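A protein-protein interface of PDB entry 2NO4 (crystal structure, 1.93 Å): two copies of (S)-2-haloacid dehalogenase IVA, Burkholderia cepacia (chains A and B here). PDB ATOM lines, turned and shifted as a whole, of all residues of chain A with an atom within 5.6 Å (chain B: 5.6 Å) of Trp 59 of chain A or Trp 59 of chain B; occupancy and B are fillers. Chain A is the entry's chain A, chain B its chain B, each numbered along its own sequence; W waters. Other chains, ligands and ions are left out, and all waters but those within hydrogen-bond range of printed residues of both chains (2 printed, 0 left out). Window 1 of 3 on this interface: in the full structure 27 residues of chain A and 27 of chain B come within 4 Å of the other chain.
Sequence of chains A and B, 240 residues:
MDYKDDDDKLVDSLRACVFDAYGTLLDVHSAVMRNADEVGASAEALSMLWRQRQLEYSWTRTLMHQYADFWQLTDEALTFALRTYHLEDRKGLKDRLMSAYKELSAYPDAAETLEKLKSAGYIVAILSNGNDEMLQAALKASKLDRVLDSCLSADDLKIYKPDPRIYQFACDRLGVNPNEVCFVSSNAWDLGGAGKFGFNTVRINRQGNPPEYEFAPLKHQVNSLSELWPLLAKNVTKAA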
ATOM      1  N   GLN A  52      24.980 -34.574 -21.783  1.00  0.00           N
ATOM      2  CA  GLN A  52      24.332 -33.281 -21.522  1.00  0.00           C
ATOM      3  C   GLN A  52      23.029 -33.430 -20.734  1.00  0.00           C
ATOM      4  O   GLN A  52      22.722 -32.625 -19.864  1.00  0.00           O
ATOM      5  CB  GLN A  52      23.964 -32.610 -22.872  1.00  0.00           C
ATOM      6  CG  GLN A  52      23.238 -31.226 -22.749  1.00  0.00           C
ATOM      7  CD  GLN A  52      21.715 -31.285 -22.578  1.00  0.00           C
ATOM      8  OE1 GLN A  52      21.066 -32.123 -23.175  1.00  0.00           O
ATOM      9  NE2 GLN A  52      21.132 -30.304 -21.814  1.00  0.00           N
ATOM     10  N   GLN A  54      22.210 -36.053 -18.655  1.00  0.00           N
ATOM     11  CA  GLN A  54      22.593 -36.525 -17.323  1.00  0.00           C
ATOM     12  C   GLN A  54      22.902 -35.309 -16.423  1.00  0.00           C
ATOM     13  O   GLN A  54      22.365 -35.191 -15.304  1.00  0.00           O
ATOM     14  CB  GLN A  54      23.794 -37.454 -17.417  1.00  0.00           C
ATOM     15  CG  GLN A  54      24.415 -37.863 -16.072  1.00  0.00           C
ATOM     16  CD  GLN A  54      25.845 -38.343 -16.239  1.00  0.00           C
ATOM     17  OE1 GLN A  54      26.676 -37.618 -16.789  1.00  0.00           O
ATOM     18  NE2 GLN A  54      26.144 -39.592 -15.787  1.00  0.00           N
ATOM     19  N   LEU A  55      23.703 -34.387 -16.938  1.00  0.00           N
ATOM     20  CA  LEU A  55      24.036 -33.167 -16.212  1.00  0.00           C
ATOM     21  C   LEU A  55      22.865 -32.196 -16.085  1.00  0.00           C
ATOM     22  O   LEU A  55      22.632 -31.700 -15.002  1.00  0.00           O
ATOM     23  CB  LEU A  55      25.238 -32.471 -16.848  1.00  0.00           C
ATOM     24  CG  LEU A  55      26.544 -33.242 -16.652  1.00  0.00           C
ATOM     25  CD1 LEU A  55      27.647 -32.543 -17.434  1.00  0.00           C
ATOM     26  CD2 LEU A  55      26.942 -33.464 -15.158  1.00  0.00           C
ATOM     27  N   GLU A  56      22.133 -31.954 -17.183  1.00  0.00           N
ATOM     28  CA  GLU A  56      20.894 -31.157 -17.151  1.00  0.00           C
ATOM     29  C   GLU A  56      19.981 -31.634 -16.014  1.00  0.00           C
ATOM     30  O   GLU A  56      19.509 -30.813 -15.208  1.00  0.00           O
ATOM     31  CB  GLU A  56      20.133 -31.209 -18.494  1.00  0.00           C
ATOM     32  CG  GLU A  56      18.682 -30.719 -18.330  1.00  0.00           C
ATOM     33  CD  GLU A  56      17.855 -30.700 -19.599  1.00  0.00           C
ATOM     34  OE1 GLU A  56      18.389 -30.388 -20.674  1.00  0.00           O
ATOM     35  OE2 GLU A  56      16.640 -30.973 -19.503  1.00  0.00           O
ATOM     36  N   TYR A  57      19.774 -32.962 -15.918  1.00  0.00           N
ATOM     37  CA  TYR A  57      18.839 -33.514 -14.943  1.00  0.00           C
ATOM     38  C   TYR A  57      19.362 -33.257 -13.528  1.00  0.00           C
ATOM     39  O   TYR A  57      18.565 -32.953 -12.641  1.00  0.00           O
ATOM     40  CB  TYR A  57      18.579 -35.013 -15.146  1.00  0.00           C
ATOM     41  CG  TYR A  57      17.913 -35.427 -16.467  1.00  0.00           C
ATOM     42  CD1 TYR A  57      17.132 -34.527 -17.211  1.00  0.00           C
ATOM     43  CD2 TYR A  57      18.056 -36.735 -16.941  1.00  0.00           C
ATOM     44  CE1 TYR A  57      16.515 -34.924 -18.426  1.00  0.00           C
ATOM     45  CE2 TYR A  57      17.430 -37.155 -18.155  1.00  0.00           C
ATOM     46  CZ  TYR A  57      16.679 -36.231 -18.873  1.00  0.00           C
ATOM     47  OH  TYR A  57      16.110 -36.611 -20.053  1.00  0.00           O
ATOM     48  N   SER A  58      20.676 -33.369 -13.332  1.00  0.00           N
ATOM     49  CA  SER A  58      21.278 -33.149 -12.003  1.00  0.00           C
ATOM     50  C   SER A  58      21.009 -31.691 -11.547  1.00  0.00           C
ATOM     51  O   SER A  58      20.597 -31.452 -10.377  1.00  0.00           O
ATOM     52  CB  SER A  58      22.793 -33.510 -11.964  1.00  0.00           C
ATOM     53  OG  SER A  58      23.616 -32.498 -12.528  1.00  0.00           O
ATOM     54  N   TRP A  59      21.154 -30.754 -12.497  1.00  0.00           N
ATOM     55  CA  TRP A  59      20.976 -29.321 -12.193  1.00  0.00           C
ATOM     56  C   TRP A  59      19.515 -28.944 -12.013  1.00  0.00           C
ATOM     57  O   TRP A  59      19.153 -28.337 -11.004  1.00  0.00           O
ATOM     58  CB  TRP A  59      21.609 -28.412 -13.241  1.00  0.00           C
ATOM     59  CG  TRP A  59      23.094 -28.646 -13.415  1.00  0.00           C
ATOM     60  CD1 TRP A  59      24.004 -28.905 -12.427  1.00  0.00           C
ATOM     61  CD2 TRP A  59      23.817 -28.684 -14.652  1.00  0.00           C
ATOM     62  NE1 TRP A  59      25.262 -29.077 -12.966  1.00  0.00           N
ATOM     63  CE2 TRP A  59      25.172 -28.947 -14.335  1.00  0.00           C
ATOM     64  CE3 TRP A  59      23.449 -28.516 -16.010  1.00  0.00           C
ATOM     65  CZ2 TRP A  59      26.167 -29.054 -15.332  1.00  0.00           C
ATOM     66  CZ3 TRP A  59      24.435 -28.624 -16.991  1.00  0.00           C
ATOM     67  CH2 TRP A  59      25.776 -28.889 -16.647  1.00  0.00           C
ATOM     68  N   THR A  60      18.686 -29.258 -13.009  1.00  0.00           N
ATOM     69  CA  THR A  60      17.305 -28.852 -12.945  1.00  0.00           C
ATOM     70  C   THR A  60      16.554 -29.531 -11.813  1.00  0.00           C
ATOM     71  O   THR A  60      15.692 -28.923 -11.212  1.00  0.00           O
ATOM     72  CB  THR A  60      16.575 -29.115 -14.279  1.00  0.00           C
ATOM     73  OG1 THR A  60      16.581 -30.509 -14.522  1.00  0.00           O
ATOM     74  CG2 THR A  60      17.235 -28.341 -15.464  1.00  0.00           C
ATOM     75  N   ARG A  61      16.849 -30.804 -11.517  1.00  0.00           N
ATOM     76  CA  ARG A  61      16.152 -31.484 -10.423  1.00  0.00           C
ATOM     77  C   ARG A  61      16.526 -30.903  -9.062  1.00  0.00           C
ATOM     78  O   ARG A  61      15.726 -30.913  -8.146  1.00  0.00           O
ATOM     79  CB  ARG A  61      16.435 -32.978 -10.412  1.00  0.00           C
ATOM     80  CG  ARG A  61      15.551 -33.792 -11.394  1.00  0.00           C
ATOM     81  CD  ARG A  61      16.118 -35.186 -11.390  1.00  0.00           C
ATOM     82  NE  ARG A  61      15.326 -36.210 -12.048  1.00  0.00           N
ATOM     83  CZ  ARG A  61      14.389 -36.959 -11.464  1.00  0.00           C
ATOM     84  NH1 ARG A  61      14.012 -36.768 -10.199  1.00  0.00           N
ATOM     85  NH2 ARG A  61      13.789 -37.881 -12.184  1.00  0.00           N
ATOM     86  N   THR A  62      17.751 -30.418  -8.923  1.00  0.00           N
ATOM     87  CA  THR A  62      18.134 -29.747  -7.675  1.00  0.00           C
ATOM     88  C   THR A  62      17.380 -28.414  -7.518  1.00  0.00           C
ATOM     89  O   THR A  62      16.819 -28.128  -6.462  1.00  0.00           O
ATOM     90  CB  THR A  62      19.650 -29.494  -7.619  1.00  0.00           C
ATOM     91  OG1 THR A  62      20.317 -30.740  -7.654  1.00  0.00           O
ATOM     92  CG2 THR A  62      20.075 -28.798  -6.256  1.00  0.00           C
ATOM     93  N   LEU A  63      17.334 -27.642  -8.598  1.00  0.00           N
ATOM     94  CA  LEU A  63      16.599 -26.366  -8.622  1.00  0.00           C
ATOM     95  C   LEU A  63      15.113 -26.516  -8.302  1.00  0.00           C
ATOM     96  O   LEU A  63      14.521 -25.670  -7.656  1.00  0.00           O
ATOM     97  CB  LEU A  63      16.805 -25.710  -9.994  1.00  0.00           C
ATOM     98  CG  LEU A  63      18.207 -25.070 -10.188  1.00  0.00           C
ATOM     99  CD1 LEU A  63      18.370 -24.667 -11.649  1.00  0.00           C
ATOM    100  CD2 LEU A  63      18.376 -23.841  -9.260  1.00  0.00           C
ATOM    101  N   MET A  64      14.503 -27.603  -8.759  1.00  0.00           N
ATOM    102  CA  MET A  64      13.098 -27.772  -8.560  1.00  0.00           C
ATOM    103  C   MET A  64      12.782 -28.669  -7.349  1.00  0.00           C
ATOM    104  O   MET A  64      11.622 -28.930  -7.066  1.00  0.00           O
ATOM    105  CB  MET A  64      12.409 -28.238  -9.878  1.00  0.00           C
ATOM    106  CG  MET A  64      12.590 -29.739 -10.174  1.00  0.00           C
ATOM    107  SD  MET A  64      11.689 -30.188 -11.708  1.00  0.00           S
ATOM    108  CE  MET A  64      12.739 -29.701 -13.027  1.00  0.00           C
ATOM    109  N   TYR A 160      22.868 -31.794  -5.643  1.00  0.00           N
ATOM    110  CA  TYR A 160      23.975 -31.901  -6.602  1.00  0.00           C
ATOM    111  C   TYR A 160      24.881 -30.673  -6.661  1.00  0.00           C
ATOM    112  O   TYR A 160      24.483 -29.563  -6.237  1.00  0.00           O
ATOM    113  CB  TYR A 160      23.416 -32.193  -8.015  1.00  0.00           C
ATOM    114  CG  TYR A 160      22.962 -33.618  -8.166  1.00  0.00           C
ATOM    115  CD1 TYR A 160      21.627 -33.917  -8.414  1.00  0.00           C
ATOM    116  CD2 TYR A 160      23.885 -34.668  -8.097  1.00  0.00           C
ATOM    117  CE1 TYR A 160      21.218 -35.227  -8.598  1.00  0.00           C
ATOM    118  CE2 TYR A 160      23.480 -36.015  -8.288  1.00  0.00           C
ATOM    119  CZ  TYR A 160      22.157 -36.269  -8.544  1.00  0.00           C
ATOM    120  OH  TYR A 160      21.723 -37.570  -8.719  1.00  0.00           O
ATOM    121  N   LYS A 161      26.103 -30.874  -7.168  1.00  0.00           N
ATOM    122  CA  LYS A 161      26.960 -29.735  -7.627  1.00  0.00           C
ATOM    123  C   LYS A 161      26.192 -28.898  -8.668  1.00  0.00           C
ATOM    124  O   LYS A 161      25.402 -29.458  -9.442  1.00  0.00           O
ATOM    125  CB  LYS A 161      28.239 -30.281  -8.300  1.00  0.00           C
ATOM    126  CG  LYS A 161      29.203 -31.044  -7.379  1.00  0.00           C
ATOM    127  CD  LYS A 161      30.098 -31.952  -8.226  1.00  0.00           C
ATOM    128  CE  LYS A 161      31.336 -32.373  -7.473  1.00  0.00           C
ATOM    129  NZ  LYS A 161      32.289 -33.046  -8.419  1.00  0.00           N
ATOM    130  N   PRO A 162      26.466 -27.567  -8.756  1.00  0.00           N
ATOM    131  CA  PRO A 162      27.430 -26.808  -7.943  1.00  0.00           C
ATOM    132  C   PRO A 162      26.843 -26.085  -6.712  1.00  0.00           C
ATOM    133  O   PRO A 162      27.332 -25.006  -6.348  1.00  0.00           O
ATOM    134  CB  PRO A 162      27.979 -25.800  -8.946  1.00  0.00           C
ATOM    135  CG  PRO A 162      26.797 -25.469  -9.814  1.00  0.00           C
ATOM    136  CD  PRO A 162      25.900 -26.738  -9.834  1.00  0.00           C
ATOM    137  N   TRP A 189      31.883 -26.064 -15.037  1.00  0.00           N
ATOM    138  CA  TRP A 189      30.818 -25.789 -14.041  1.00  0.00           C
ATOM    139  C   TRP A 189      31.190 -26.168 -12.585  1.00  0.00           C
ATOM    140  O   TRP A 189      30.817 -25.470 -11.643  1.00  0.00           O
ATOM    141  CB  TRP A 189      29.463 -26.419 -14.445  1.00  0.00           C
ATOM    142  CG  TRP A 189      29.536 -27.885 -14.780  1.00  0.00           C
ATOM    143  CD1 TRP A 189      29.756 -28.440 -16.019  1.00  0.00           C
ATOM    144  CD2 TRP A 189      29.461 -28.978 -13.854  1.00  0.00           C
ATOM    145  NE1 TRP A 189      29.814 -29.817 -15.916  1.00  0.00           N
ATOM    146  CE2 TRP A 189      29.615 -30.178 -14.609  1.00  0.00           C
ATOM    147  CE3 TRP A 189      29.230 -29.071 -12.468  1.00  0.00           C
ATOM    148  CZ2 TRP A 189      29.567 -31.463 -14.012  1.00  0.00           C
ATOM    149  CZ3 TRP A 189      29.189 -30.371 -11.867  1.00  0.00           C
ATOM    150  CH2 TRP A 189      29.362 -31.533 -12.646  1.00  0.00           C
ATOM    151  N   GLN B  52      22.566 -25.006 -25.507  1.00  0.00           N
ATOM    152  CA  GLN B  52      22.860 -25.873 -24.374  1.00  0.00           C
ATOM    153  C   GLN B  52      23.624 -25.124 -23.270  1.00  0.00           C
ATOM    154  O   GLN B  52      23.301 -25.273 -22.077  1.00  0.00           O
ATOM    155  CB  GLN B  52      23.674 -27.136 -24.818  1.00  0.00           C
ATOM    156  CG  GLN B  52      23.988 -28.156 -23.623  1.00  0.00           C
ATOM    157  CD  GLN B  52      25.223 -27.771 -22.723  1.00  0.00           C
ATOM    158  OE1 GLN B  52      26.227 -27.273 -23.242  1.00  0.00           O
ATOM    159  NE2 GLN B  52      25.157 -28.066 -21.385  1.00  0.00           N
ATOM    160  N   GLN B  54      23.831 -21.796 -22.859  1.00  0.00           N
ATOM    161  CA  GLN B  54      22.994 -20.684 -22.351  1.00  0.00           C
ATOM    162  C   GLN B  54      22.155 -21.189 -21.174  1.00  0.00           C
ATOM    163  O   GLN B  54      22.105 -20.549 -20.111  1.00  0.00           O
ATOM    164  CB  GLN B  54      22.128 -20.099 -23.459  1.00  0.00           C
ATOM    165  CG  GLN B  54      21.008 -19.099 -23.054  1.00  0.00           C
ATOM    166  CD  GLN B  54      19.951 -18.985 -24.149  1.00  0.00           C
ATOM    167  OE1 GLN B  54      19.311 -19.983 -24.503  1.00  0.00           O
ATOM    168  NE2 GLN B  54      19.777 -17.758 -24.722  1.00  0.00           N
ATOM    169  N   LEU B  55      21.532 -22.351 -21.376  1.00  0.00           N
ATOM    170  CA  LEU B  55      20.699 -22.994 -20.396  1.00  0.00           C
ATOM    171  C   LEU B  55      21.535 -23.530 -19.280  1.00  0.00           C
ATOM    172  O   LEU B  55      21.196 -23.290 -18.133  1.00  0.00           O
ATOM    173  CB  LEU B  55      19.856 -24.115 -21.035  1.00  0.00           C
ATOM    174  CG  LEU B  55      18.726 -23.554 -21.912  1.00  0.00           C
ATOM    175  CD1 LEU B  55      17.948 -24.723 -22.480  1.00  0.00           C
ATOM    176  CD2 LEU B  55      17.855 -22.542 -21.135  1.00  0.00           C
ATOM    177  N   GLU B  56      22.630 -24.254 -19.590  1.00  0.00           N
ATOM    178  CA  GLU B  56      23.553 -24.667 -18.525  1.00  0.00           C
ATOM    179  C   GLU B  56      23.901 -23.500 -17.578  1.00  0.00           C
ATOM    180  O   GLU B  56      23.825 -23.665 -16.356  1.00  0.00           O
ATOM    181  CB  GLU B  56      24.873 -25.210 -19.081  1.00  0.00           C
ATOM    182  CG  GLU B  56      25.940 -25.329 -17.978  1.00  0.00           C
ATOM    183  CD  GLU B  56      27.240 -25.970 -18.451  1.00  0.00           C
ATOM    184  OE1 GLU B  56      27.198 -26.851 -19.329  1.00  0.00           O
ATOM    185  OE2 GLU B  56      28.320 -25.598 -17.946  1.00  0.00           O
ATOM    186  N   TYR B  57      24.340 -22.372 -18.149  1.00  0.00           N
ATOM    187  CA  TYR B  57      24.733 -21.193 -17.358  1.00  0.00           C
ATOM    188  C   TYR B  57      23.615 -20.711 -16.464  1.00  0.00           C
ATOM    189  O   TYR B  57      23.869 -20.307 -15.347  1.00  0.00           O
ATOM    190  CB  TYR B  57      25.256 -20.016 -18.226  1.00  0.00           C
ATOM    191  CG  TYR B  57      26.507 -20.338 -18.993  1.00  0.00           C
ATOM    192  CD1 TYR B  57      27.333 -21.411 -18.624  1.00  0.00           C
ATOM    193  CD2 TYR B  57      26.848 -19.593 -20.137  1.00  0.00           C
ATOM    194  CE1 TYR B  57      28.526 -21.713 -19.401  1.00  0.00           C
ATOM    195  CE2 TYR B  57      28.027 -19.860 -20.902  1.00  0.00           C
ATOM    196  CZ  TYR B  57      28.839 -20.903 -20.536  1.00  0.00           C
ATOM    197  OH  TYR B  57      29.984 -21.114 -21.307  1.00  0.00           O
ATOM    198  N   SER B  58      22.378 -20.747 -16.959  1.00  0.00           N
ATOM    199  CA  SER B  58      21.256 -20.316 -16.157  1.00  0.00           C
ATOM    200  C   SER B  58      21.030 -21.243 -14.945  1.00  0.00           C
ATOM    201  O   SER B  58      20.760 -20.765 -13.867  1.00  0.00           O
ATOM    202  CB  SER B  58      19.988 -20.132 -17.032  1.00  0.00           C
ATOM    203  OG  SER B  58      19.299 -21.379 -17.274  1.00  0.00           O
ATOM    204  N   TRP B  59      21.163 -22.568 -15.120  1.00  0.00           N
ATOM    205  CA  TRP B  59      20.967 -23.504 -14.031  1.00  0.00           C
ATOM    206  C   TRP B  59      22.133 -23.466 -13.023  1.00  0.00           C
ATOM    207  O   TRP B  59      21.899 -23.368 -11.828  1.00  0.00           O
ATOM    208  CB  TRP B  59      20.740 -24.921 -14.565  1.00  0.00           C
ATOM    209  CG  TRP B  59      19.583 -25.016 -15.540  1.00  0.00           C
ATOM    210  CD1 TRP B  59      18.371 -24.371 -15.468  1.00  0.00           C
ATOM    211  CD2 TRP B  59      19.542 -25.807 -16.730  1.00  0.00           C
ATOM    212  NE1 TRP B  59      17.576 -24.725 -16.539  1.00  0.00           N
ATOM    213  CE2 TRP B  59      18.268 -25.600 -17.328  1.00  0.00           C
ATOM    214  CE3 TRP B  59      20.465 -26.692 -17.353  1.00  0.00           C
ATOM    215  CZ2 TRP B  59      17.891 -26.216 -18.532  1.00  0.00           C
ATOM    216  CZ3 TRP B  59      20.090 -27.304 -18.550  1.00  0.00           C
ATOM    217  CH2 TRP B  59      18.812 -27.076 -19.120  1.00  0.00           C
ATOM    218  N   THR B  60      23.377 -23.537 -13.501  1.00  0.00           N
ATOM    219  CA  THR B  60      24.495 -23.683 -12.590  1.00  0.00           C
ATOM    220  C   THR B  60      24.741 -22.371 -11.794  1.00  0.00           C
ATOM    221  O   THR B  60      25.103 -22.433 -10.634  1.00  0.00           O
ATOM    222  CB  THR B  60      25.762 -24.136 -13.309  1.00  0.00           C
ATOM    223  OG1 THR B  60      26.093 -23.158 -14.286  1.00  0.00           O
ATOM    224  CG2 THR B  60      25.521 -25.526 -14.013  1.00  0.00           C
ATOM    225  N   ARG B  61      24.570 -21.223 -12.443  1.00  0.00           N
ATOM    226  CA  ARG B  61      24.739 -19.920 -11.778  1.00  0.00           C
ATOM    227  C   ARG B  61      23.702 -19.689 -10.691  1.00  0.00           C
ATOM    228  O   ARG B  61      24.012 -19.139  -9.631  1.00  0.00           O
ATOM    229  CB  ARG B  61      24.674 -18.794 -12.789  1.00  0.00           C
ATOM    230  CG  ARG B  61      25.986 -18.548 -13.512  1.00  0.00           C
ATOM    231  CD  ARG B  61      25.706 -17.501 -14.605  1.00  0.00           C
ATOM    232  NE  ARG B  61      26.907 -16.954 -15.266  1.00  0.00           N
ATOM    233  CZ  ARG B  61      27.625 -15.914 -14.831  1.00  0.00           C
ATOM    234  NH1 ARG B  61      27.364 -15.352 -13.642  1.00  0.00           N
ATOM    235  NH2 ARG B  61      28.638 -15.487 -15.568  1.00  0.00           N
ATOM    236  N   THR B  62      22.478 -20.149 -10.902  1.00  0.00           N
ATOM    237  CA  THR B  62      21.557 -20.081  -9.766  1.00  0.00           C
ATOM    238  C   THR B  62      21.904 -21.022  -8.624  1.00  0.00           C
ATOM    239  O   THR B  62      21.824 -20.631  -7.442  1.00  0.00           O
ATOM    240  CB  THR B  62      20.008 -19.837 -10.073  1.00  0.00           C
ATOM    241  OG1 THR B  62      19.131 -20.668  -9.278  1.00  0.00           O
ATOM    242  CG2 THR B  62      19.667 -19.792 -11.466  1.00  0.00           C
ATOM    243  N   LEU B  63      22.361 -22.228  -8.975  1.00  0.00           N
ATOM    244  CA  LEU B  63      22.782 -23.222  -7.956  1.00  0.00           C
ATOM    245  C   LEU B  63      23.981 -22.754  -7.156  1.00  0.00           C
ATOM    246  O   LEU B  63      24.054 -23.031  -5.968  1.00  0.00           O
ATOM    247  CB  LEU B  63      23.080 -24.589  -8.596  1.00  0.00           C
ATOM    248  CG  LEU B  63      21.830 -25.385  -9.019  1.00  0.00           C
ATOM    249  CD1 LEU B  63      22.188 -26.588  -9.851  1.00  0.00           C
ATOM    250  CD2 LEU B  63      20.988 -25.766  -7.770  1.00  0.00           C
ATOM    251  N   MET B  64      24.929 -22.078  -7.803  1.00  0.00           N
ATOM    252  CA  MET B  64      26.100 -21.587  -7.078  1.00  0.00           C
ATOM    253  C   MET B  64      25.959 -20.107  -6.633  1.00  0.00           C
ATOM    254  O   MET B  64      26.927 -19.504  -6.161  1.00  0.00           O
ATOM    255  CB  MET B  64      27.401 -21.802  -7.871  1.00  0.00           C
ATOM    256  CG  MET B  64      27.598 -20.878  -9.091  1.00  0.00           C
ATOM    257  SD  MET B  64      29.136 -21.131 -10.011  1.00  0.00           S
ATOM    258  CE  MET B  64      28.739 -22.513 -11.114  1.00  0.00           C
ATOM    259  N   TYR B 160      16.579 -18.131 -11.769  1.00  0.00           N
ATOM    260  CA  TYR B 160      16.133 -18.745 -13.025  1.00  0.00           C
ATOM    261  C   TYR B 160      15.206 -19.943 -12.830  1.00  0.00           C
ATOM    262  O   TYR B 160      15.209 -20.571 -11.779  1.00  0.00           O
ATOM    263  CB  TYR B 160      17.356 -19.163 -13.840  1.00  0.00           C
ATOM    264  CG  TYR B 160      18.054 -18.007 -14.525  1.00  0.00           C
ATOM    265  CD1 TYR B 160      19.365 -17.670 -14.203  1.00  0.00           C
ATOM    266  CD2 TYR B 160      17.402 -17.270 -15.534  1.00  0.00           C
ATOM    267  CE1 TYR B 160      20.013 -16.644 -14.874  1.00  0.00           C
ATOM    268  CE2 TYR B 160      18.055 -16.257 -16.205  1.00  0.00           C
ATOM    269  CZ  TYR B 160      19.339 -15.951 -15.867  1.00  0.00           C
ATOM    270  OH  TYR B 160      19.969 -14.938 -16.502  1.00  0.00           O
ATOM    271  N   LYS B 161      14.417 -20.250 -13.858  1.00  0.00           N
ATOM    272  CA  LYS B 161      13.660 -21.498 -13.904  1.00  0.00           C
ATOM    273  C   LYS B 161      14.677 -22.659 -13.820  1.00  0.00           C
ATOM    274  O   LYS B 161      15.814 -22.500 -14.281  1.00  0.00           O
ATOM    275  CB  LYS B 161      12.923 -21.591 -15.244  1.00  0.00           C
ATOM    276  CG  LYS B 161      11.844 -20.572 -15.463  1.00  0.00           C
ATOM    277  CD  LYS B 161      11.557 -20.531 -16.966  1.00  0.00           C
ATOM    278  CE  LYS B 161      10.255 -19.838 -17.278  1.00  0.00           C
ATOM    279  NZ  LYS B 161       9.921 -20.018 -18.762  1.00  0.00           N
ATOM    280  N   PRO B 162      14.258 -23.836 -13.312  1.00  0.00           N
ATOM    281  CA  PRO B 162      12.905 -24.190 -12.798  1.00  0.00           C
ATOM    282  C   PRO B 162      12.727 -24.037 -11.273  1.00  0.00           C
ATOM    283  O   PRO B 162      11.996 -24.823 -10.658  1.00  0.00           O
ATOM    284  CB  PRO B 162      12.789 -25.677 -13.172  1.00  0.00           C
ATOM    285  CG  PRO B 162      14.211 -26.197 -13.152  1.00  0.00           C
ATOM    286  CD  PRO B 162      15.155 -25.019 -13.338  1.00  0.00           C
ATOM    287  N   TRP B 189      12.200 -29.234 -19.073  1.00  0.00           N
ATOM    288  CA  TRP B 189      12.672 -28.884 -17.727  1.00  0.00           C
ATOM    289  C   TRP B 189      11.756 -27.784 -17.086  1.00  0.00           C
ATOM    290  O   TRP B 189      11.534 -27.760 -15.893  1.00  0.00           O
ATOM    291  CB  TRP B 189      14.175 -28.437 -17.777  1.00  0.00           C
ATOM    292  CG  TRP B 189      14.486 -27.442 -18.839  1.00  0.00           C
ATOM    293  CD1 TRP B 189      14.946 -27.722 -20.092  1.00  0.00           C
ATOM    294  CD2 TRP B 189      14.292 -26.005 -18.794  1.00  0.00           C
ATOM    295  NE1 TRP B 189      15.060 -26.575 -20.828  1.00  0.00           N
ATOM    296  CE2 TRP B 189      14.671 -25.501 -20.065  1.00  0.00           C
ATOM    297  CE3 TRP B 189      13.843 -25.099 -17.803  1.00  0.00           C
ATOM    298  CZ2 TRP B 189      14.602 -24.123 -20.408  1.00  0.00           C
ATOM    299  CZ3 TRP B 189      13.774 -23.695 -18.150  1.00  0.00           C
ATOM    300  CH2 TRP B 189      14.163 -23.241 -19.435  1.00  0.00           C
HETATM  301  O   HOH W   1      23.284 -29.921 -20.067  1.00  0.00           O
HETATM  302  O   HOH W   2      22.331 -27.641 -20.992  1.00  0.00           O
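Hydrophobic or aromatic side chains of chain A within 4 Å of the printed part of chain B: Trp 59, Leu 63, Met 64, Pro 162 and Trp 189.
Along chain A the printed residues that touch a printed residue of chain B span positions 52 to 189.
Of the 16 printed residues of chain B, 9 touch a printed residue of chain A.
Printed residues of chain B that touch a printed residue of chain A: Gln 52, Glu 56, Trp 59, Thr 60, Thr 62, Leu 63, Met 64, Pro 162 and Trp 189.
Among the printed residues, no Asp or Glu carboxylate lies within 4 Å of a Lys or Arg side-chain nitrogen of the other chain.
NE2 of Gln 52 of chain B is in hydrogen-bond range of OE1 of Glu 56 of chain B (3.1 Å).
The backbone carbonyl oxygen (O) of Glu 56 of chain A is in hydrogen-bond range of the side-chain hydroxyl (OG1) of Thr 60 of chain A (3.0 Å).
The side-chain hydroxyl of Thr 62 of chain A is in hydrogen-bond range of the backbone NH of Tyr 160 of chain A, 3.4 Å away.
Water W1 bridges O of Gln 52 of chain A and NE2 of Gln 52 of chain B.
Water W2 lies within hydrogen-bond range of the backbone carbonyl oxygen of Gln 52 of chain B (2.8 Å) and the side-chain amide nitrogen of Gln 52 of chain A (3.0 Å).
Trp 59 of chain A touches Thr 60 of chain B, and with the chains exchanged Thr 60 of chain A touches Trp 59 of chain B.
Of the 22 pairs that touch across the chains among the printed residues, 21 have their exchanged pair printed and touching as well.
Of the printed residues of chain B, Gln 52 of chain A touches Gln 52 (3.3 Å).
Of chain B, only Glu 56 (3.7 Å), Trp 59 (3.7 Å), Thr 60 (3.5 Å) and Leu 63 (3.7 Å) come within 4 Å of Trp 59 of chain A.
Of the printed residues of chain A, Trp 59 of chain B touches Glu 56 (3.7 Å), Trp 59 (3.7 Å), Thr 60 (3.5 Å) and Leu 63 (3.7 Å).
Printed residues of chain A within 4 Å of Pro 162 of chain B: Thr 60, Leu 63 and Met 64.
Among the printed residues, pairs that only touch across the chains: Leu 63 of chain A with Thr 62 of chain B (3.3 Å), Gln 52 of chain A with Gln 52 of chain B (3.3 Å), Trp 59 of chain A with Thr 60 of chain B (3.5 Å), Thr 60 of chain A with Trp 59 of chain B (3.5 Å), Thr 62 of chain A with Leu 63 of chain B (3.5 Å), Met 64 of chain A with Pro 162 of chain B (3.5 Å), Pro 162 of chain A with Met 64 of chain B (3.5 Å), Leu 63 of chain A with Leu 63 of chain B (3.6 Å), Pro 162 of chain A with Thr 60 of chain B (3.6 Å), Leu 63 of chain A with Pro 162 of chain B (3.6 Å), Trp 189 of chain A with Met 64 of chain B (3.7 Å), Trp 59 of chain A with Glu 56 of chain B (3.7 Å), Thr 60 of chain A with Pro 162 of chain B (3.7 Å), Met 64 of chain A with Trp 189 of chain B (3.7 Å), Glu 56 of chain A with Trp 59 of chain B (3.7 Å), Trp 59 of chain A with Leu 63 of chain B (3.7 Å), Leu 63 of chain A with Trp 59 of chain B (3.7 Å), Glu 56 of chain A with Trp 189 of chain B (3.7 Å), Pro 162 of chain A with Leu 63 of chain B (3.7 Å), Trp 189 of chain A with Glu 56 of chain B (3.7 Å), Trp 59 of chain A with Trp 59 of chain B (3.7 Å) and Thr 60 of chain A with Trp 189 of chain B (3.8 Å).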
